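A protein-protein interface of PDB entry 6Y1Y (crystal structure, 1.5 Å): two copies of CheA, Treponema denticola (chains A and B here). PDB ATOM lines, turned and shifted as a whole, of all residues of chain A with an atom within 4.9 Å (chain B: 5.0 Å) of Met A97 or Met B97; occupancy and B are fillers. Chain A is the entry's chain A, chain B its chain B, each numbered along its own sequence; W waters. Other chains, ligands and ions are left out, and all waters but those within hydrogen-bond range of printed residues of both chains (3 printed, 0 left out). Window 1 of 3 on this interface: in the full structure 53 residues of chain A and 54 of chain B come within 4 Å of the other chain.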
ATOM      1  N   PHE A  34      21.620 -28.325  -5.693  1.00  0.00           N
ATOM      2  CA  PHE A  34      22.337 -27.228  -6.334  1.00  0.00           C
ATOM      3  C   PHE A  34      21.512 -25.948  -6.360  1.00  0.00           C
ATOM      4  O   PHE A  34      22.081 -24.861  -6.242  1.00  0.00           O
ATOM      5  CB  PHE A  34      22.807 -27.655  -7.724  1.00  0.00           C
ATOM      6  CG  PHE A  34      24.044 -28.510  -7.672  1.00  0.00           C
ATOM      7  CD1 PHE A  34      25.286 -27.938  -7.431  1.00  0.00           C
ATOM      8  CD2 PHE A  34      23.961 -29.889  -7.795  1.00  0.00           C
ATOM      9  CE1 PHE A  34      26.429 -28.727  -7.343  1.00  0.00           C
ATOM     10  CE2 PHE A  34      25.099 -30.682  -7.703  1.00  0.00           C
ATOM     11  CZ  PHE A  34      26.339 -30.090  -7.481  1.00  0.00           C
ATOM     12  N   LEU A  37      22.128 -24.478  -3.082  1.00  0.00           N
ATOM     13  CA  LEU A  37      23.465 -23.893  -3.050  1.00  0.00           C
ATOM     14  C   LEU A  37      23.504 -22.561  -3.785  1.00  0.00           C
ATOM     15  O   LEU A  37      24.137 -21.613  -3.308  1.00  0.00           O
ATOM     16  CB  LEU A  37      24.470 -24.868  -3.656  1.00  0.00           C
ATOM     17  CG  LEU A  37      24.795 -26.039  -2.729  1.00  0.00           C
ATOM     18  CD1 LEU A  37      25.512 -27.143  -3.480  1.00  0.00           C
ATOM     19  CD2 LEU A  37      25.635 -25.547  -1.574  1.00  0.00           C
ATOM     20  N   TYR A  38      22.810 -22.456  -4.923  1.00  0.00           N
ATOM     21  CA  TYR A  38      22.712 -21.151  -5.574  1.00  0.00           C
ATOM     22  C   TYR A  38      22.079 -20.127  -4.624  1.00  0.00           C
ATOM     23  O   TYR A  38      22.589 -19.012  -4.475  1.00  0.00           O
ATOM     24  CB  TYR A  38      21.931 -21.228  -6.890  1.00  0.00           C
ATOM     25  CG  TYR A  38      21.492 -19.838  -7.254  1.00  0.00           C
ATOM     26  CD1 TYR A  38      22.417 -18.887  -7.661  1.00  0.00           C
ATOM     27  CD2 TYR A  38      20.169 -19.455  -7.107  1.00  0.00           C
ATOM     28  CE1 TYR A  38      22.023 -17.583  -7.939  1.00  0.00           C
ATOM     29  CE2 TYR A  38      19.767 -18.163  -7.377  1.00  0.00           C
ATOM     30  CZ  TYR A  38      20.701 -17.233  -7.794  1.00  0.00           C
ATOM     31  OH  TYR A  38      20.292 -15.936  -8.062  1.00  0.00           O
ATOM     32  N   ASP A  92      28.955 -22.734   5.198  1.00  0.00           N
ATOM     33  CA  ASP A  92      29.410 -24.023   4.706  1.00  0.00           C
ATOM     34  C   ASP A  92      29.237 -24.183   3.205  1.00  0.00           C
ATOM     35  O   ASP A  92      29.227 -25.316   2.720  1.00  0.00           O
ATOM     36  CB  ASP A  92      28.664 -25.154   5.415  1.00  0.00           C
ATOM     37  CG  ASP A  92      28.900 -25.170   6.913  1.00  0.00           C
ATOM     38  OD1 ASP A  92      29.950 -24.680   7.383  1.00  0.00           O
ATOM     39  OD2 ASP A  92      28.024 -25.682   7.630  1.00  0.00           O
ATOM     40  N   PHE A  93      29.142 -23.087   2.449  1.00  0.00           N
ATOM     41  CA  PHE A  93      28.914 -23.224   1.014  1.00  0.00           C
ATOM     42  C   PHE A  93      29.919 -24.176   0.372  1.00  0.00           C
ATOM     43  O   PHE A  93      29.537 -25.065  -0.399  1.00  0.00           O
ATOM     44  CB  PHE A  93      28.994 -21.859   0.321  1.00  0.00           C
ATOM     45  CG  PHE A  93      28.832 -21.947  -1.169  1.00  0.00           C
ATOM     46  CD1 PHE A  93      27.560 -22.000  -1.737  1.00  0.00           C
ATOM     47  CD2 PHE A  93      29.934 -22.042  -2.001  1.00  0.00           C
ATOM     48  CE1 PHE A  93      27.386 -22.115  -3.105  1.00  0.00           C
ATOM     49  CE2 PHE A  93      29.773 -22.170  -3.379  1.00  0.00           C
ATOM     50  CZ  PHE A  93      28.497 -22.198  -3.937  1.00  0.00           C
ATOM     51  N   ASP A  94      31.208 -24.000   0.662  1.00  0.00           N
ATOM     52  CA  ASP A  94      32.205 -24.801  -0.042  1.00  0.00           C
ATOM     53  C   ASP A  94      32.098 -26.292   0.287  1.00  0.00           C
ATOM     54  O   ASP A  94      32.165 -27.126  -0.622  1.00  0.00           O
ATOM     55  CB  ASP A  94      33.605 -24.262   0.239  1.00  0.00           C
ATOM     56  CG  ASP A  94      34.061 -24.533   1.632  1.00  0.00           C
ATOM     57  OD1 ASP A  94      33.448 -23.989   2.578  1.00  0.00           O
ATOM     58  OD2 ASP A  94      35.025 -25.313   1.786  1.00  0.00           O
ATOM     59  N   SER A  95      31.918 -26.654   1.562  1.00  0.00           N
ATOM     60  CA  SER A  95      31.841 -28.076   1.908  1.00  0.00           C
ATOM     61  C   SER A  95      30.547 -28.699   1.401  1.00  0.00           C
ATOM     62  O   SER A  95      30.540 -29.850   0.935  1.00  0.00           O
ATOM     63  CB  SER A  95      32.001 -28.269   3.413  1.00  0.00           C
ATOM     64  OG  SER A  95      31.088 -27.474   4.130  1.00  0.00           O
ATOM     65  N   LEU A  96      29.438 -27.962   1.499  1.00  0.00           N
ATOM     66  CA  LEU A  96      28.180 -28.438   0.931  1.00  0.00           C
ATOM     67  C   LEU A  96      28.295 -28.605  -0.579  1.00  0.00           C
ATOM     68  O   LEU A  96      27.810 -29.592  -1.151  1.00  0.00           O
ATOM     69  CB  LEU A  96      27.049 -27.458   1.281  1.00  0.00           C
ATOM     70  CG  LEU A  96      26.683 -27.367   2.766  1.00  0.00           C
ATOM     71  CD1 LEU A  96      25.844 -26.121   3.068  1.00  0.00           C
ATOM     72  CD2 LEU A  96      25.949 -28.624   3.220  1.00  0.00           C
ATOM     73  N   MET A  97      28.932 -27.642  -1.252  1.00  0.00           N
ATOM     74  CA  MET A  97      29.110 -27.748  -2.693  1.00  0.00           C
ATOM     75  C   MET A  97      29.954 -28.960  -3.062  1.00  0.00           C
ATOM     76  O   MET A  97      29.615 -29.699  -3.991  1.00  0.00           O
ATOM     77  CB  MET A  97      29.738 -26.472  -3.239  1.00  0.00           C
ATOM     78  CG  MET A  97      29.963 -26.546  -4.720  1.00  0.00           C
ATOM     79  SD  MET A  97      28.489 -26.002  -5.597  1.00  0.00           S
ATOM     80  CE  MET A  97      29.201 -25.565  -7.205  1.00  0.00           C
ATOM     81  N   LYS A  98      31.072 -29.171  -2.358  1.00  0.00           N
ATOM     82  CA  LYS A  98      31.926 -30.309  -2.681  1.00  0.00           C
ATOM     83  C   LYS A  98      31.171 -31.621  -2.525  1.00  0.00           C
ATOM     84  O   LYS A  98      31.284 -32.516  -3.371  1.00  0.00           O
ATOM     85  CB  LYS A  98      33.179 -30.308  -1.804  1.00  0.00           C
ATOM     86  CG  LYS A  98      34.249 -31.284  -2.295  1.00  0.00           C
ATOM     87  CD  LYS A  98      35.419 -31.345  -1.335  1.00  0.00           C
ATOM     88  CE  LYS A  98      36.460 -32.334  -1.837  1.00  0.00           C
ATOM     89  NZ  LYS A  98      37.677 -32.339  -0.977  1.00  0.00           N
ATOM     90  N   ALA A  99      30.397 -31.757  -1.451  1.00  0.00           N
ATOM     91  CA  ALA A  99      29.622 -32.977  -1.269  1.00  0.00           C
ATOM     92  C   ALA A  99      28.591 -33.144  -2.375  1.00  0.00           C
ATOM     93  O   ALA A  99      28.377 -34.256  -2.872  1.00  0.00           O
ATOM     94  CB  ALA A  99      28.944 -32.960   0.100  1.00  0.00           C
ATOM     95  N   ALA A 100      27.934 -32.051  -2.771  1.00  0.00           N
ATOM     96  CA  ALA A 100      26.909 -32.149  -3.803  1.00  0.00           C
ATOM     97  C   ALA A 100      27.513 -32.522  -5.146  1.00  0.00           C
ATOM     98  O   ALA A 100      26.904 -33.280  -5.915  1.00  0.00           O
ATOM     99  CB  ALA A 100      26.129 -30.836  -3.898  1.00  0.00           C
ATOM    100  N   VAL A 101      28.705 -31.993  -5.447  1.00  0.00           N
ATOM    101  CA  VAL A 101      29.390 -32.361  -6.682  1.00  0.00           C
ATOM    102  C   VAL A 101      29.748 -33.842  -6.670  1.00  0.00           C
ATOM    103  O   VAL A 101      29.553 -34.553  -7.665  1.00  0.00           O
ATOM    104  CB  VAL A 101      30.633 -31.475  -6.876  1.00  0.00           C
ATOM    105  CG1 VAL A 101      31.477 -32.002  -8.024  1.00  0.00           C
ATOM    106  CG2 VAL A 101      30.210 -30.037  -7.145  1.00  0.00           C
ATOM    107  N   PHE B  34      29.922 -27.729 -12.486  1.00  0.00           N
ATOM    108  CA  PHE B  34      29.870 -27.470 -11.053  1.00  0.00           C
ATOM    109  C   PHE B  34      31.224 -27.704 -10.395  1.00  0.00           C
ATOM    110  O   PHE B  34      31.551 -27.034  -9.411  1.00  0.00           O
ATOM    111  CB  PHE B  34      28.788 -28.319 -10.385  1.00  0.00           C
ATOM    112  CG  PHE B  34      27.389 -27.836 -10.651  1.00  0.00           C
ATOM    113  CD1 PHE B  34      26.983 -26.573 -10.231  1.00  0.00           C
ATOM    114  CD2 PHE B  34      26.470 -28.661 -11.290  1.00  0.00           C
ATOM    115  CE1 PHE B  34      25.695 -26.127 -10.476  1.00  0.00           C
ATOM    116  CE2 PHE B  34      25.184 -28.221 -11.545  1.00  0.00           C
ATOM    117  CZ  PHE B  34      24.794 -26.954 -11.134  1.00  0.00           C
ATOM    118  N   LEU B  37      32.977 -24.537 -10.953  1.00  0.00           N
ATOM    119  CA  LEU B  37      32.432 -23.512 -10.068  1.00  0.00           C
ATOM    120  C   LEU B  37      32.917 -23.697  -8.635  1.00  0.00           C
ATOM    121  O   LEU B  37      33.188 -22.712  -7.936  1.00  0.00           O
ATOM    122  CB  LEU B  37      30.905 -23.528 -10.141  1.00  0.00           C
ATOM    123  CG  LEU B  37      30.328 -22.857 -11.394  1.00  0.00           C
ATOM    124  CD1 LEU B  37      28.862 -23.205 -11.584  1.00  0.00           C
ATOM    125  CD2 LEU B  37      30.499 -21.347 -11.289  1.00  0.00           C
ATOM    126  N   TYR B  38      33.024 -24.940  -8.165  1.00  0.00           N
ATOM    127  CA  TYR B  38      33.603 -25.169  -6.846  1.00  0.00           C
ATOM    128  C   TYR B  38      35.024 -24.618  -6.780  1.00  0.00           C
ATOM    129  O   TYR B  38      35.383 -23.900  -5.838  1.00  0.00           O
ATOM    130  CB  TYR B  38      33.583 -26.672  -6.511  1.00  0.00           C
ATOM    131  CG  TYR B  38      34.367 -27.025  -5.264  1.00  0.00           C
ATOM    132  CD1 TYR B  38      33.848 -26.783  -3.997  1.00  0.00           C
ATOM    133  CD2 TYR B  38      35.640 -27.573  -5.352  1.00  0.00           C
ATOM    134  CE1 TYR B  38      34.580 -27.086  -2.854  1.00  0.00           C
ATOM    135  CE2 TYR B  38      36.373 -27.876  -4.217  1.00  0.00           C
ATOM    136  CZ  TYR B  38      35.836 -27.639  -2.972  1.00  0.00           C
ATOM    137  OH  TYR B  38      36.580 -27.936  -1.845  1.00  0.00           O
ATOM    138  N   ASP B  92      30.951 -12.568 -11.674  1.00  0.00           N
ATOM    139  CA  ASP B  92      29.619 -13.006 -12.046  1.00  0.00           C
ATOM    140  C   ASP B  92      29.291 -14.397 -11.522  1.00  0.00           C
ATOM    141  O   ASP B  92      28.447 -15.077 -12.112  1.00  0.00           O
ATOM    142  CB  ASP B  92      29.461 -12.978 -13.564  1.00  0.00           C
ATOM    143  CG  ASP B  92      29.527 -11.574 -14.130  1.00  0.00           C
ATOM    144  OD1 ASP B  92      28.948 -10.652 -13.510  1.00  0.00           O
ATOM    145  OD2 ASP B  92      30.170 -11.386 -15.185  1.00  0.00           O
ATOM    146  N   PHE B  93      29.942 -14.833 -10.442  1.00  0.00           N
ATOM    147  CA  PHE B  93      29.697 -16.177  -9.919  1.00  0.00           C
ATOM    148  C   PHE B  93      28.212 -16.454  -9.729  1.00  0.00           C
ATOM    149  O   PHE B  93      27.736 -17.540 -10.064  1.00  0.00           O
ATOM    150  CB  PHE B  93      30.435 -16.389  -8.593  1.00  0.00           C
ATOM    151  CG  PHE B  93      30.435 -17.829  -8.124  1.00  0.00           C
ATOM    152  CD1 PHE B  93      29.384 -18.330  -7.356  1.00  0.00           C
ATOM    153  CD2 PHE B  93      31.479 -18.679  -8.455  1.00  0.00           C
ATOM    154  CE1 PHE B  93      29.378 -19.660  -6.933  1.00  0.00           C
ATOM    155  CE2 PHE B  93      31.474 -20.006  -8.028  1.00  0.00           C
ATOM    156  CZ  PHE B  93      30.429 -20.494  -7.280  1.00  0.00           C
ATOM    157  N   ASP B  94      27.465 -15.501  -9.159  1.00  0.00           N
ATOM    158  CA  ASP B  94      26.064 -15.793  -8.858  1.00  0.00           C
ATOM    159  C   ASP B  94      25.296 -16.141 -10.134  1.00  0.00           C
ATOM    160  O   ASP B  94      24.519 -17.102 -10.147  1.00  0.00           O
ATOM    161  CB  ASP B  94      25.397 -14.640  -8.076  1.00  0.00           C
ATOM    162  CG  ASP B  94      25.599 -13.252  -8.695  1.00  0.00           C
ATOM    163  OD1 ASP B  94      26.160 -13.102  -9.793  1.00  0.00           O
ATOM    164  OD2 ASP B  94      25.174 -12.266  -8.046  1.00  0.00           O
ATOM    165  N   SER B  95      25.545 -15.408 -11.222  1.00  0.00           N
ATOM    166  CA  SER B  95      24.881 -15.662 -12.501  1.00  0.00           C
ATOM    167  C   SER B  95      25.341 -16.971 -13.128  1.00  0.00           C
ATOM    168  O   SER B  95      24.524 -17.731 -13.663  1.00  0.00           O
ATOM    169  CB  SER B  95      25.163 -14.508 -13.466  1.00  0.00           C
ATOM    170  OG  SER B  95      24.283 -13.432 -13.234  1.00  0.00           O
ATOM    171  N   LEU B  96      26.648 -17.247 -13.072  1.00  0.00           N
ATOM    172  CA  LEU B  96      27.191 -18.491 -13.612  1.00  0.00           C
ATOM    173  C   LEU B  96      26.645 -19.706 -12.871  1.00  0.00           C
ATOM    174  O   LEU B  96      26.306 -20.725 -13.494  1.00  0.00           O
ATOM    175  CB  LEU B  96      28.714 -18.478 -13.539  1.00  0.00           C
ATOM    176  CG  LEU B  96      29.441 -17.415 -14.356  1.00  0.00           C
ATOM    177  CD1 LEU B  96      30.922 -17.478 -14.035  1.00  0.00           C
ATOM    178  CD2 LEU B  96      29.193 -17.631 -15.842  1.00  0.00           C
ATOM    179  N   MET B  97      26.569 -19.624 -11.537  1.00  0.00           N
ATOM    180  CA  MET B  97      26.000 -20.712 -10.743  1.00  0.00           C
ATOM    181  C   MET B  97      24.532 -20.924 -11.085  1.00  0.00           C
ATOM    182  O   MET B  97      24.087 -22.060 -11.295  1.00  0.00           O
ATOM    183  CB  MET B  97      26.175 -20.408  -9.255  1.00  0.00           C
ATOM    184  CG  MET B  97      25.598 -21.459  -8.361  1.00  0.00           C
ATOM    185  SD  MET B  97      26.728 -22.847  -8.243  1.00  0.00           S
ATOM    186  CE  MET B  97      25.821 -23.850  -7.062  1.00  0.00           C
ATOM    187  N   LYS B  98      23.761 -19.835 -11.164  1.00  0.00           N
ATOM    188  CA  LYS B  98      22.346 -19.980 -11.486  1.00  0.00           C
ATOM    189  C   LYS B  98      22.156 -20.626 -12.854  1.00  0.00           C
ATOM    190  O   LYS B  98      21.317 -21.514 -13.018  1.00  0.00           O
ATOM    191  CB  LYS B  98      21.642 -18.622 -11.435  1.00  0.00           C
ATOM    192  CG  LYS B  98      20.128 -18.802 -11.436  1.00  0.00           C
ATOM    193  CD  LYS B  98      19.374 -17.497 -11.281  1.00  0.00           C
ATOM    194  CE  LYS B  98      17.888 -17.798 -11.223  1.00  0.00           C
ATOM    195  NZ  LYS B  98      17.049 -16.569 -11.114  1.00  0.00           N
ATOM    196  N   ALA B  99      22.928 -20.197 -13.847  1.00  0.00           N
ATOM    197  CA  ALA B  99      22.802 -20.790 -15.176  1.00  0.00           C
ATOM    198  C   ALA B  99      23.149 -22.273 -15.156  1.00  0.00           C
ATOM    199  O   ALA B  99      22.517 -23.070 -15.854  1.00  0.00           O
ATOM    200  CB  ALA B  99      23.682 -20.033 -16.174  1.00  0.00           C
ATOM    201  N   ALA B 100      24.156 -22.657 -14.370  1.00  0.00           N
ATOM    202  CA  ALA B 100      24.521 -24.065 -14.296  1.00  0.00           C
ATOM    203  C   ALA B 100      23.400 -24.887 -13.672  1.00  0.00           C
ATOM    204  O   ALA B 100      23.119 -26.008 -14.128  1.00  0.00           O
ATOM    205  CB  ALA B 100      25.819 -24.229 -13.506  1.00  0.00           C
ATOM    206  N   VAL B 101      22.732 -24.343 -12.641  1.00  0.00           N
ATOM    207  CA  VAL B 101      21.587 -25.031 -12.038  1.00  0.00           C
ATOM    208  C   VAL B 101      20.461 -25.172 -13.051  1.00  0.00           C
ATOM    209  O   VAL B 101      19.864 -26.246 -13.194  1.00  0.00           O
ATOM    210  CB  VAL B 101      21.104 -24.294 -10.768  1.00  0.00           C
ATOM    211  CG1 VAL B 101      19.825 -24.951 -10.226  1.00  0.00           C
ATOM    212  CG2 VAL B 101      22.198 -24.283  -9.698  1.00  0.00           C
HETATM  213  O   HOH W   1      38.728 -29.645  -2.080  1.00  0.00           O
HETATM  214  O   HOH W   2      35.401 -27.950   0.699  1.00  0.00           O
HETATM  215  O   HOH W   3      17.273 -15.601  -8.394  1.00  0.00           O
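Water W1 bridges the side-chain hydroxyl (OH) of Tyr B38 (2.8 Å) and the side-chain amino group (NZ) of Lys A98 (3.1 Å).
Water W2 bridges the side-chain hydroxyl of Tyr B38 (2.8 Å) and the side-chain carboxylate of Asp A94 (2.9 Å).
Water W3 lies within hydrogen-bond range of NZ of Lys B98 and OH of Tyr A38.
Printed residues of chain B within 4 Å of Phe A34: Phe B34 (3.5 Å), Met B97 (3.96 Å) and Val B101 (3.5 Å).
Of the printed residues of chain B, Leu A37 touches Met B97 (3.8 Å).
Phe A93 touches none of the printed residues of chain B.
Of the printed residues of chain B, Asp A94 touches Tyr B38.
Met A97 touches just these residues of chain B: Phe B34 (3.5 Å), Leu B37 (3.96 Å), Tyr B38 (3.96 Å) and Met B97 (3.7 Å).
Of chain A, only Phe A34 (3.96 Å), Leu A37 (3.8 Å), Tyr A38 (3.9 Å) and Met A97 (3.7 Å) come within 4 Å of Met B97.
Ala B99 touches none of the printed residues of chain A.
The nearest residue of chain A that does not touch Met B97 is Phe A93 (4.4 Å).
The nearest printed residue of chain A that does not touch Tyr B38 is Val A101 (4.8 Å).
Phe B34 touches its own counterpart, Phe A34.
Phe A34 touches Met B97, and with the chains exchanged Met A97 touches Phe B34.
Tyr A38 touches Met B97, and with the chains exchanged Met A97 touches Tyr B38.
Met A97 touches its own counterpart, Met B97.
Of the 14 pairs that touch across the chains among the printed residues, 14 have their exchanged pair printed and touching as well.
Phe A34 touches Met B97.
O of Phe A34 touches CG2 of Val B101 (3.5 Å).
Met B97 touches Leu A37.
Asp B94 touches Tyr A38.
Tyr A38 touches Met B97 (N to CE, 3.9 Å).
CE1 of Tyr A38 touches CB of Lys B98, at 3.7 Å.
Asp A94 touches Tyr B38.
CB of Leu B37 touches CE of Met A97, 3.96 Å away.
CG of Met A97 touches CD1 of Tyr B38 (3.96 Å).
CE of Met B97 touches SD of Met A97, at 3.7 Å.
Of the 13 printed residues of chain B, 7 touch a printed residue of chain A.
Printed residues of chain B that touch a printed residue of chain A: Phe B34, Leu B37, Tyr B38, Asp B94, Met B97, Lys B98 and Val B101.
Hydrophobic or aromatic side chains of chain B that line the printed part of chain A: Phe B34, Leu B37, Tyr B38, Met B97 and Val B101.
Along chain B the printed residues that touch a printed residue of chain A span positions 34 to 101.
Of the 13 printed residues of chain A, 7 touch a printed residue of chain B.
Among the printed residues, 14 pairs touch across the chains.
Among the printed residues, no Asp or Glu carboxylate lies within 4 Å of a Lys or Arg side-chain nitrogen of the other chain.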
